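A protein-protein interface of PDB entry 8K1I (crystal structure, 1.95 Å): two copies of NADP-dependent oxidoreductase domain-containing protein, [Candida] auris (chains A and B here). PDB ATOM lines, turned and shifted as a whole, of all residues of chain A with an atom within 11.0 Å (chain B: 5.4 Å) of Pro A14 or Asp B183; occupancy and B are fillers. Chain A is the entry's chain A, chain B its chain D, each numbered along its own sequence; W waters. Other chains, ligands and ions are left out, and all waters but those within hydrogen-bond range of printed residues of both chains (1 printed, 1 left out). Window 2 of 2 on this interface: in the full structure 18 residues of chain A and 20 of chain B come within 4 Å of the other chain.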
ATOM      1  N   PRO A   8      28.404  23.870 -25.911  1.00  0.00           N
ATOM      2  CA  PRO A   8      27.376  23.916 -26.961  1.00  0.00           C
ATOM      3  C   PRO A   8      26.390  25.058 -26.738  1.00  0.00           C
ATOM      4  O   PRO A   8      26.220  25.567 -25.629  1.00  0.00           O
ATOM      5  CB  PRO A   8      26.673  22.551 -26.849  1.00  0.00           C
ATOM      6  CG  PRO A   8      27.014  22.048 -25.491  1.00  0.00           C
ATOM      7  CD  PRO A   8      28.355  22.620 -25.137  1.00  0.00           C
ATOM      8  N   ARG A  10      23.057  24.777 -27.620  1.00  0.00           N
ATOM      9  CA  ARG A  10      21.799  24.062 -27.827  1.00  0.00           C
ATOM     10  C   ARG A  10      21.484  23.285 -26.552  1.00  0.00           C
ATOM     11  O   ARG A  10      22.245  23.337 -25.579  1.00  0.00           O
ATOM     12  CB  ARG A  10      21.900  23.112 -29.027  1.00  0.00           C
ATOM     13  CG  ARG A  10      22.926  21.998 -28.814  1.00  0.00           C
ATOM     14  CD  ARG A  10      23.276  21.244 -30.092  1.00  0.00           C
ATOM     15  NE  ARG A  10      23.255  19.794 -29.886  1.00  0.00           N
ATOM     16  CZ  ARG A  10      23.166  18.893 -30.857  1.00  0.00           C
ATOM     17  NH1 ARG A  10      23.161  19.250 -32.131  1.00  0.00           N
ATOM     18  NH2 ARG A  10      23.092  17.599 -30.541  1.00  0.00           N
ATOM     19  N   VAL A  11      20.375  22.532 -26.562  1.00  0.00           N
ATOM     20  CA  VAL A  11      20.029  21.635 -25.458  1.00  0.00           C
ATOM     21  C   VAL A  11      20.313  20.219 -25.948  1.00  0.00           C
ATOM     22  O   VAL A  11      19.670  19.736 -26.888  1.00  0.00           O
ATOM     23  CB  VAL A  11      18.574  21.812 -24.989  1.00  0.00           C
ATOM     24  CG1 VAL A  11      18.188  20.740 -24.007  1.00  0.00           C
ATOM     25  CG2 VAL A  11      18.394  23.200 -24.307  1.00  0.00           C
ATOM     26  N   LEU A  12      21.309  19.567 -25.343  1.00  0.00           N
ATOM     27  CA  LEU A  12      21.743  18.256 -25.835  1.00  0.00           C
ATOM     28  C   LEU A  12      20.618  17.234 -25.798  1.00  0.00           C
ATOM     29  O   LEU A  12      19.737  17.263 -24.925  1.00  0.00           O
ATOM     30  CB  LEU A  12      22.914  17.712 -25.017  1.00  0.00           C
ATOM     31  CG  LEU A  12      24.312  18.271 -25.292  1.00  0.00           C
ATOM     32  CD1 LEU A  12      25.379  17.253 -24.894  1.00  0.00           C
ATOM     33  CD2 LEU A  12      24.477  18.657 -26.741  1.00  0.00           C
ATOM     34  N   GLN A  13      20.683  16.294 -26.748  1.00  0.00           N
ATOM     35  CA  GLN A  13      19.822  15.133 -26.827  1.00  0.00           C
ATOM     36  C   GLN A  13      20.652  13.878 -26.658  1.00  0.00           C
ATOM     37  O   GLN A  13      21.734  13.788 -27.240  1.00  0.00           O
ATOM     38  CB  GLN A  13      19.057  15.050 -28.165  1.00  0.00           C
ATOM     39  CG  GLN A  13      17.642  15.616 -28.104  1.00  0.00           C
ATOM     40  CD  GLN A  13      16.649  14.684 -27.379  1.00  0.00           C
ATOM     41  OE1 GLN A  13      15.823  15.132 -26.582  1.00  0.00           O
ATOM     42  NE2 GLN A  13      16.707  13.386 -27.694  1.00  0.00           N
ATOM     43  N   PRO A  14      20.174  12.892 -25.865  1.00  0.00           N
ATOM     44  CA  PRO A  14      18.914  12.903 -25.103  1.00  0.00           C
ATOM     45  C   PRO A  14      18.963  13.938 -23.986  1.00  0.00           C
ATOM     46  O   PRO A  14      20.038  14.365 -23.581  1.00  0.00           O
ATOM     47  CB  PRO A  14      18.824  11.477 -24.565  1.00  0.00           C
ATOM     48  CG  PRO A  14      20.260  11.096 -24.368  1.00  0.00           C
ATOM     49  CD  PRO A  14      20.965  11.686 -25.571  1.00  0.00           C
ATOM     50  N   TYR A  15      17.817  14.387 -23.497  1.00  0.00           N
ATOM     51  CA  TYR A  15      17.796  15.450 -22.503  1.00  0.00           C
ATOM     52  C   TYR A  15      18.376  14.973 -21.170  1.00  0.00           C
ATOM     53  O   TYR A  15      18.129  13.853 -20.742  1.00  0.00           O
ATOM     54  CB  TYR A  15      16.359  15.934 -22.298  1.00  0.00           C
ATOM     55  CG  TYR A  15      16.264  17.075 -21.338  1.00  0.00           C
ATOM     56  CD1 TYR A  15      16.215  16.850 -19.978  1.00  0.00           C
ATOM     57  CD2 TYR A  15      16.236  18.392 -21.793  1.00  0.00           C
ATOM     58  CE1 TYR A  15      16.152  17.903 -19.093  1.00  0.00           C
ATOM     59  CE2 TYR A  15      16.162  19.446 -20.920  1.00  0.00           C
ATOM     60  CZ  TYR A  15      16.123  19.194 -19.558  1.00  0.00           C
ATOM     61  OH  TYR A  15      16.042  20.233 -18.644  1.00  0.00           O
ATOM     62  N   SER A  16      19.112  15.864 -20.482  1.00  0.00           N
ATOM     63  CA  SER A  16      19.529  15.612 -19.101  1.00  0.00           C
ATOM     64  C   SER A  16      19.831  16.917 -18.376  1.00  0.00           C
ATOM     65  O   SER A  16      20.542  17.779 -18.906  1.00  0.00           O
ATOM     66  CB  SER A  16      20.771  14.720 -19.049  1.00  0.00           C
ATOM     67  OG  SER A  16      21.147  14.484 -17.702  1.00  0.00           O
ATOM     68  N   ILE A  17      19.326  17.040 -17.149  1.00  0.00           N
ATOM     69  CA  ILE A  17      19.632  18.223 -16.344  1.00  0.00           C
ATOM     70  C   ILE A  17      21.134  18.370 -16.084  1.00  0.00           C
ATOM     71  O   ILE A  17      21.583  19.457 -15.712  1.00  0.00           O
ATOM     72  CB  ILE A  17      18.810  18.210 -15.030  1.00  0.00           C
ATOM     73  CG1 ILE A  17      18.569  19.617 -14.480  1.00  0.00           C
ATOM     74  CG2 ILE A  17      19.463  17.350 -13.971  1.00  0.00           C
ATOM     75  CD1 ILE A  17      17.961  20.611 -15.431  1.00  0.00           C
ATOM     76  N   VAL A  18      21.935  17.322 -16.311  1.00  0.00           N
ATOM     77  CA  VAL A  18      23.358  17.471 -16.039  1.00  0.00           C
ATOM     78  C   VAL A  18      24.029  18.263 -17.157  1.00  0.00           C
ATOM     79  O   VAL A  18      25.167  18.724 -16.983  1.00  0.00           O
ATOM     80  CB  VAL A  18      24.090  16.129 -15.852  1.00  0.00           C
ATOM     81  CG1 VAL A  18      23.401  15.262 -14.757  1.00  0.00           C
ATOM     82  CG2 VAL A  18      24.277  15.411 -17.193  1.00  0.00           C
ATOM     83  N   ASN A  19      23.347  18.465 -18.298  1.00  0.00           N
ATOM     84  CA  ASN A  19      23.890  19.320 -19.352  1.00  0.00           C
ATOM     85  C   ASN A  19      23.615  20.818 -19.135  1.00  0.00           C
ATOM     86  O   ASN A  19      23.879  21.596 -20.068  1.00  0.00           O
ATOM     87  CB  ASN A  19      23.371  18.917 -20.737  1.00  0.00           C
ATOM     88  CG  ASN A  19      23.586  17.432 -21.034  1.00  0.00           C
ATOM     89  OD1 ASN A  19      24.639  16.878 -20.727  1.00  0.00           O
ATOM     90  ND2 ASN A  19      22.598  16.800 -21.669  1.00  0.00           N
ATOM     91  N   LEU A  20      23.099  21.239 -17.970  1.00  0.00           N
ATOM     92  CA  LEU A  20      23.143  22.656 -17.625  1.00  0.00           C
ATOM     93  C   LEU A  20      24.585  23.141 -17.811  1.00  0.00           C
ATOM     94  O   LEU A  20      25.517  22.446 -17.383  1.00  0.00           O
ATOM     95  CB  LEU A  20      22.702  22.868 -16.175  1.00  0.00           C
ATOM     96  CG  LEU A  20      21.196  22.911 -15.882  1.00  0.00           C
ATOM     97  CD1 LEU A  20      20.895  22.904 -14.378  1.00  0.00           C
ATOM     98  CD2 LEU A  20      20.480  24.043 -16.614  1.00  0.00           C
ATOM     99  N   GLU A  85      13.458  25.840 -26.920  1.00  0.00           N
ATOM    100  CA  GLU A  85      14.231  24.603 -26.834  1.00  0.00           C
ATOM    101  C   GLU A  85      15.745  24.814 -26.841  1.00  0.00           C
ATOM    102  O   GLU A  85      16.479  23.842 -26.642  1.00  0.00           O
ATOM    103  CB  GLU A  85      13.893  23.681 -28.004  1.00  0.00           C
ATOM    104  CG  GLU A  85      14.422  24.219 -29.334  1.00  0.00           C
ATOM    105  CD  GLU A  85      13.317  24.621 -30.299  1.00  0.00           C
ATOM    106  OE1 GLU A  85      12.164  24.757 -29.846  1.00  0.00           O
ATOM    107  OE2 GLU A  85      13.610  24.839 -31.498  1.00  0.00           O
ATOM    108  N   TYR A  88      18.055  26.631 -21.152  1.00  0.00           N
ATOM    109  CA  TYR A  88      17.465  26.153 -19.912  1.00  0.00           C
ATOM    110  C   TYR A  88      16.884  27.298 -19.093  1.00  0.00           C
ATOM    111  O   TYR A  88      17.482  28.373 -19.011  1.00  0.00           O
ATOM    112  CB  TYR A  88      18.510  25.416 -19.083  1.00  0.00           C
ATOM    113  CG  TYR A  88      19.123  24.236 -19.791  1.00  0.00           C
ATOM    114  CD1 TYR A  88      20.207  24.392 -20.677  1.00  0.00           C
ATOM    115  CD2 TYR A  88      18.625  22.956 -19.582  1.00  0.00           C
ATOM    116  CE1 TYR A  88      20.786  23.269 -21.314  1.00  0.00           C
ATOM    117  CE2 TYR A  88      19.179  21.876 -20.216  1.00  0.00           C
ATOM    118  CZ  TYR A  88      20.255  22.026 -21.077  1.00  0.00           C
ATOM    119  OH  TYR A  88      20.777  20.892 -21.698  1.00  0.00           O
ATOM    120  N   ASP A 125      12.837  23.990 -16.851  1.00  0.00           N
ATOM    121  CA  ASP A 125      13.861  22.949 -16.776  1.00  0.00           C
ATOM    122  C   ASP A 125      14.104  22.498 -15.342  1.00  0.00           C
ATOM    123  O   ASP A 125      14.229  21.297 -15.083  1.00  0.00           O
ATOM    124  CB  ASP A 125      15.159  23.428 -17.426  1.00  0.00           C
ATOM    125  CG  ASP A 125      15.013  23.588 -18.924  1.00  0.00           C
ATOM    126  OD1 ASP A 125      15.135  22.581 -19.635  1.00  0.00           O
ATOM    127  OD2 ASP A 125      14.814  24.716 -19.412  1.00  0.00           O
ATOM    128  N   LYS A 157      11.182  19.581 -15.662  1.00  0.00           N
ATOM    129  CA  LYS A 157      12.085  18.523 -16.067  1.00  0.00           C
ATOM    130  C   LYS A 157      12.899  17.981 -14.900  1.00  0.00           C
ATOM    131  O   LYS A 157      13.435  16.858 -14.987  1.00  0.00           O
ATOM    132  CB  LYS A 157      13.050  19.046 -17.150  1.00  0.00           C
ATOM    133  CG  LYS A 157      12.407  19.635 -18.407  1.00  0.00           C
ATOM    134  CD  LYS A 157      11.242  18.820 -18.945  1.00  0.00           C
ATOM    135  CE  LYS A 157      11.685  17.934 -20.099  1.00  0.00           C
ATOM    136  NZ  LYS A 157      11.842  18.684 -21.414  1.00  0.00           N
ATOM    137  N   LYS A 289      39.116  19.030 -18.038  1.00  0.00           N
ATOM    138  CA  LYS A 289      37.849  18.478 -18.520  1.00  0.00           C
ATOM    139  C   LYS A 289      36.753  18.843 -17.514  1.00  0.00           C
ATOM    140  O   LYS A 289      36.873  18.539 -16.325  1.00  0.00           O
ATOM    141  CB  LYS A 289      37.962  16.954 -18.713  1.00  0.00           C
ATOM    142  CG  LYS A 289      36.900  16.323 -19.610  1.00  0.00           C
ATOM    143  CD  LYS A 289      37.047  14.789 -19.719  1.00  0.00           C
ATOM    144  CE  LYS A 289      35.784  14.133 -20.295  1.00  0.00           C
ATOM    145  NZ  LYS A 289      35.064  13.170 -19.376  1.00  0.00           N
ATOM    146  N   GLN A 292      30.607  17.520 -15.547  1.00  0.00           N
ATOM    147  CA  GLN A 292      29.241  17.931 -15.896  1.00  0.00           C
ATOM    148  C   GLN A 292      28.245  17.815 -14.746  1.00  0.00           C
ATOM    149  O   GLN A 292      27.115  18.305 -14.883  1.00  0.00           O
ATOM    150  CB  GLN A 292      28.716  17.118 -17.088  1.00  0.00           C
ATOM    151  CG  GLN A 292      29.668  17.055 -18.261  1.00  0.00           C
ATOM    152  CD  GLN A 292      30.536  15.820 -18.213  1.00  0.00           C
ATOM    153  OE1 GLN A 292      30.877  15.333 -17.120  1.00  0.00           O
ATOM    154  NE2 GLN A 292      30.852  15.258 -19.395  1.00  0.00           N
ATOM    155  N   ARG A 293      28.610  17.182 -13.635  1.00  0.00           N
ATOM    156  CA  ARG A 293      27.702  17.157 -12.502  1.00  0.00           C
ATOM    157  C   ARG A 293      27.742  18.466 -11.706  1.00  0.00           C
ATOM    158  O   ARG A 293      27.113  18.537 -10.651  1.00  0.00           O
ATOM    159  CB  ARG A 293      27.996  15.947 -11.609  1.00  0.00           C
ATOM    160  CG  ARG A 293      27.733  14.565 -12.326  1.00  0.00           C
ATOM    161  CD  ARG A 293      27.272  13.431 -11.356  1.00  0.00           C
ATOM    162  NE  ARG A 293      27.039  12.156 -12.033  1.00  0.00           N
ATOM    163  CZ  ARG A 293      25.950  11.835 -12.731  1.00  0.00           C
ATOM    164  NH1 ARG A 293      24.961  12.710 -12.939  1.00  0.00           N
ATOM    165  NH2 ARG A 293      25.864  10.616 -13.277  1.00  0.00           N
ATOM    166  N   ARG B 145      22.577   3.374 -25.323  1.00  0.00           N
ATOM    167  CA  ARG B 145      22.178   4.673 -25.862  1.00  0.00           C
ATOM    168  C   ARG B 145      20.842   4.585 -26.578  1.00  0.00           C
ATOM    169  O   ARG B 145      20.074   5.558 -26.588  1.00  0.00           O
ATOM    170  CB  ARG B 145      23.233   5.200 -26.833  1.00  0.00           C
ATOM    171  CG  ARG B 145      24.539   5.588 -26.167  1.00  0.00           C
ATOM    172  CD  ARG B 145      25.584   6.009 -27.204  1.00  0.00           C
ATOM    173  NE  ARG B 145      26.694   6.680 -26.535  1.00  0.00           N
ATOM    174  CZ  ARG B 145      27.871   6.109 -26.319  1.00  0.00           C
ATOM    175  NH1 ARG B 145      28.142   4.891 -26.765  1.00  0.00           N
ATOM    176  NH2 ARG B 145      28.795   6.769 -25.635  1.00  0.00           N
ATOM    177  N   ARG B 148      18.241   4.377 -23.801  1.00  0.00           N
ATOM    178  CA  ARG B 148      18.096   5.691 -23.173  1.00  0.00           C
ATOM    179  C   ARG B 148      17.132   6.569 -23.966  1.00  0.00           C
ATOM    180  O   ARG B 148      16.314   7.295 -23.379  1.00  0.00           O
ATOM    181  CB  ARG B 148      19.471   6.357 -23.063  1.00  0.00           C
ATOM    182  CG  ARG B 148      19.429   7.799 -22.590  1.00  0.00           C
ATOM    183  CD  ARG B 148      19.188   7.877 -21.107  1.00  0.00           C
ATOM    184  NE  ARG B 148      19.363   9.257 -20.699  1.00  0.00           N
ATOM    185  CZ  ARG B 148      18.477  10.210 -20.958  1.00  0.00           C
ATOM    186  NH1 ARG B 148      17.259   9.923 -21.394  1.00  0.00           N
ATOM    187  NH2 ARG B 148      18.822  11.484 -20.790  1.00  0.00           N
ATOM    188  N   LEU B 149      17.205   6.486 -25.307  1.00  0.00           N
ATOM    189  CA  LEU B 149      16.255   7.161 -26.196  1.00  0.00           C
ATOM    190  C   LEU B 149      14.850   6.557 -26.121  1.00  0.00           C
ATOM    191  O   LEU B 149      13.867   7.298 -26.111  1.00  0.00           O
ATOM    192  CB  LEU B 149      16.758   7.131 -27.642  1.00  0.00           C
ATOM    193  CG  LEU B 149      18.118   7.776 -27.961  1.00  0.00           C
ATOM    194  CD1 LEU B 149      18.352   7.692 -29.440  1.00  0.00           C
ATOM    195  CD2 LEU B 149      18.233   9.256 -27.480  1.00  0.00           C
ATOM    196  N   GLU B 152      13.454   8.106 -23.157  1.00  0.00           N
ATOM    197  CA  GLU B 152      12.991   9.464 -23.410  1.00  0.00           C
ATOM    198  C   GLU B 152      11.708   9.468 -24.227  1.00  0.00           C
ATOM    199  O   GLU B 152      10.816  10.287 -23.985  1.00  0.00           O
ATOM    200  CB  GLU B 152      14.070  10.271 -24.115  1.00  0.00           C
ATOM    201  CG  GLU B 152      13.822  11.741 -24.016  1.00  0.00           C
ATOM    202  CD  GLU B 152      14.915  12.511 -24.668  1.00  0.00           C
ATOM    203  OE1 GLU B 152      14.867  12.629 -25.913  1.00  0.00           O
ATOM    204  OE2 GLU B 152      15.819  12.991 -23.941  1.00  0.00           O
ATOM    205  N   TYR B 180      30.210   8.477 -19.838  1.00  0.00           N
ATOM    206  CA  TYR B 180      29.105   8.596 -20.778  1.00  0.00           C
ATOM    207  C   TYR B 180      27.907   9.281 -20.152  1.00  0.00           C
ATOM    208  O   TYR B 180      26.758   8.940 -20.459  1.00  0.00           O
ATOM    209  CB  TYR B 180      28.711   7.219 -21.297  1.00  0.00           C
ATOM    210  CG  TYR B 180      29.804   6.537 -22.072  1.00  0.00           C
ATOM    211  CD1 TYR B 180      30.546   7.231 -23.036  1.00  0.00           C
ATOM    212  CD2 TYR B 180      30.145   5.223 -21.809  1.00  0.00           C
ATOM    213  CE1 TYR B 180      31.560   6.599 -23.751  1.00  0.00           C
ATOM    214  CE2 TYR B 180      31.162   4.592 -22.510  1.00  0.00           C
ATOM    215  CZ  TYR B 180      31.865   5.274 -23.479  1.00  0.00           C
ATOM    216  OH  TYR B 180      32.897   4.638 -24.173  1.00  0.00           O
ATOM    217  N   VAL B 181      28.156  10.222 -19.237  1.00  0.00           N
ATOM    218  CA  VAL B 181      27.040  10.791 -18.503  1.00  0.00           C
ATOM    219  C   VAL B 181      26.118  11.582 -19.431  1.00  0.00           C
ATOM    220  O   VAL B 181      24.943  11.775 -19.099  1.00  0.00           O
ATOM    221  CB  VAL B 181      27.547  11.654 -17.327  1.00  0.00           C
ATOM    222  CG1 VAL B 181      28.402  12.885 -17.840  1.00  0.00           C
ATOM    223  CG2 VAL B 181      26.387  12.063 -16.429  1.00  0.00           C
ATOM    224  N   GLU B 182      26.613  11.996 -20.616  1.00  0.00           N
ATOM    225  CA  GLU B 182      25.862  12.901 -21.489  1.00  0.00           C
ATOM    226  C   GLU B 182      24.834  12.176 -22.354  1.00  0.00           C
ATOM    227  O   GLU B 182      23.699  12.652 -22.494  1.00  0.00           O
ATOM    228  CB  GLU B 182      26.819  13.697 -22.380  1.00  0.00           C
ATOM    229  CG  GLU B 182      27.813  14.540 -21.585  1.00  0.00           C
ATOM    230  CD  GLU B 182      28.281  15.800 -22.306  1.00  0.00           C
ATOM    231  OE1 GLU B 182      27.914  16.020 -23.483  1.00  0.00           O
ATOM    232  OE2 GLU B 182      29.061  16.553 -21.692  1.00  0.00           O
ATOM    233  N   ASP B 183      25.195  11.054 -22.968  1.00  0.00           N
ATOM    234  CA  ASP B 183      24.250  10.373 -23.831  1.00  0.00           C
ATOM    235  C   ASP B 183      23.679   9.115 -23.209  1.00  0.00           C
ATOM    236  O   ASP B 183      22.790   8.510 -23.807  1.00  0.00           O
ATOM    237  CB  ASP B 183      24.872   9.995 -25.184  1.00  0.00           C
ATOM    238  CG  ASP B 183      26.287   9.458 -25.067  1.00  0.00           C
ATOM    239  OD1 ASP B 183      26.680   9.015 -23.964  1.00  0.00           O
ATOM    240  OD2 ASP B 183      27.012   9.487 -26.098  1.00  0.00           O
ATOM    241  N   ILE B 184      24.205   8.657 -22.078  1.00  0.00           N
ATOM    242  CA  ILE B 184      23.564   7.534 -21.402  1.00  0.00           C
ATOM    243  C   ILE B 184      23.109   7.951 -20.015  1.00  0.00           C
ATOM    244  O   ILE B 184      21.934   7.815 -19.691  1.00  0.00           O
ATOM    245  CB  ILE B 184      24.466   6.291 -21.328  1.00  0.00           C
ATOM    246  CG1 ILE B 184      24.750   5.774 -22.738  1.00  0.00           C
ATOM    247  CG2 ILE B 184      23.810   5.221 -20.491  1.00  0.00           C
ATOM    248  CD1 ILE B 184      25.799   4.646 -22.840  1.00  0.00           C
ATOM    249  N   GLY B 185      24.020   8.459 -19.183  1.00  0.00           N
ATOM    250  CA  GLY B 185      23.690   8.746 -17.799  1.00  0.00           C
ATOM    251  C   GLY B 185      23.603   7.492 -16.946  1.00  0.00           C
ATOM    252  O   GLY B 185      23.814   6.366 -17.407  1.00  0.00           O
HETATM  253  O   HOH W   1      22.693  12.496 -17.482  1.00  0.00           O
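Water W1 lies within hydrogen-bond range of the side-chain hydroxyl of Ser A16 (2.5 Å) and the backbone carbonyl oxygen of Val B181 (2.9 Å).
NE2 of Gln A13 is in hydrogen-bond range of OE1 of Glu B152 (2.7 Å). N of Tyr A15 sits at hydrogen-bond distance from OE2 of Glu B152 (2.5 Å). The backbone carbonyl oxygen (O) of Tyr A15 is in hydrogen-bond range of the guanidinium group (NH2) of Arg B148 (2.5 Å). The side-chain amide nitrogen of Gln A292 lies within hydrogen-bond range of the side-chain carboxylate of Glu B182 (3.2 Å).
Of the 10 printed residues of chain B, 6 touch a printed residue of chain A. Of the 19 printed residues of chain A, 6 touch a printed residue of chain B. Printed residues of chain A that touch a printed residue of chain B: Leu A12, Gln A13, Pro A14, Tyr A15, Gln A292 and Arg A293. Among the printed residues, 11 pairs touch across the chains.
No position is printed for both chains.
Of chain A, only Pro A14 (3.7 Å) comes within 4 Å of Asp B183. Leu B149 touches one residue of chain A. Of chain A, only Gln A292 (3.6 Å) and Arg A293 (3.5 Å) come within 4 Å of Val B181. Glu B182 touches two residues of chain A. No residue of chain A comes within 4 Å of Gly B185. Printed residues of chain B within 4 Å of Gln A292: Val B181 and Glu B182. Of the printed residues of chain B, Leu A12 touches Glu B182. Ser A16 touches none of the printed residues of chain B. The nearest printed residue of chain B that does not touch Arg A293 is Gly B185 (5.3 Å).
Glu B182 touches Leu A12 (OE1 to CD1, 3.2 Å). Arg B148 touches Pro A14. Pro A14 touches Leu B149 (CB to CD2, 3.7 Å). Pro A14 touches Glu B152 (C to OE2, 3.3 Å). Pro A14 touches Asp B183 (CG to O, 3.7 Å). Gln A292 touches Val B181. Arg A293 touches Val B181.
The guanidinium group (NE) of Arg B145 lies within salt-bridge range of the side-chain carboxylate (OD2) of Asp B183, at 2.9 Å. The side-chain carboxylate of Asp A125 sits at hydrogen-bond distance from the side-chain hydroxyl of Tyr A15, at 2.7 Å. The guanidinium group (NE) of Arg B148 lies close to the backbone carbonyl oxygen (O) of Ile B184.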
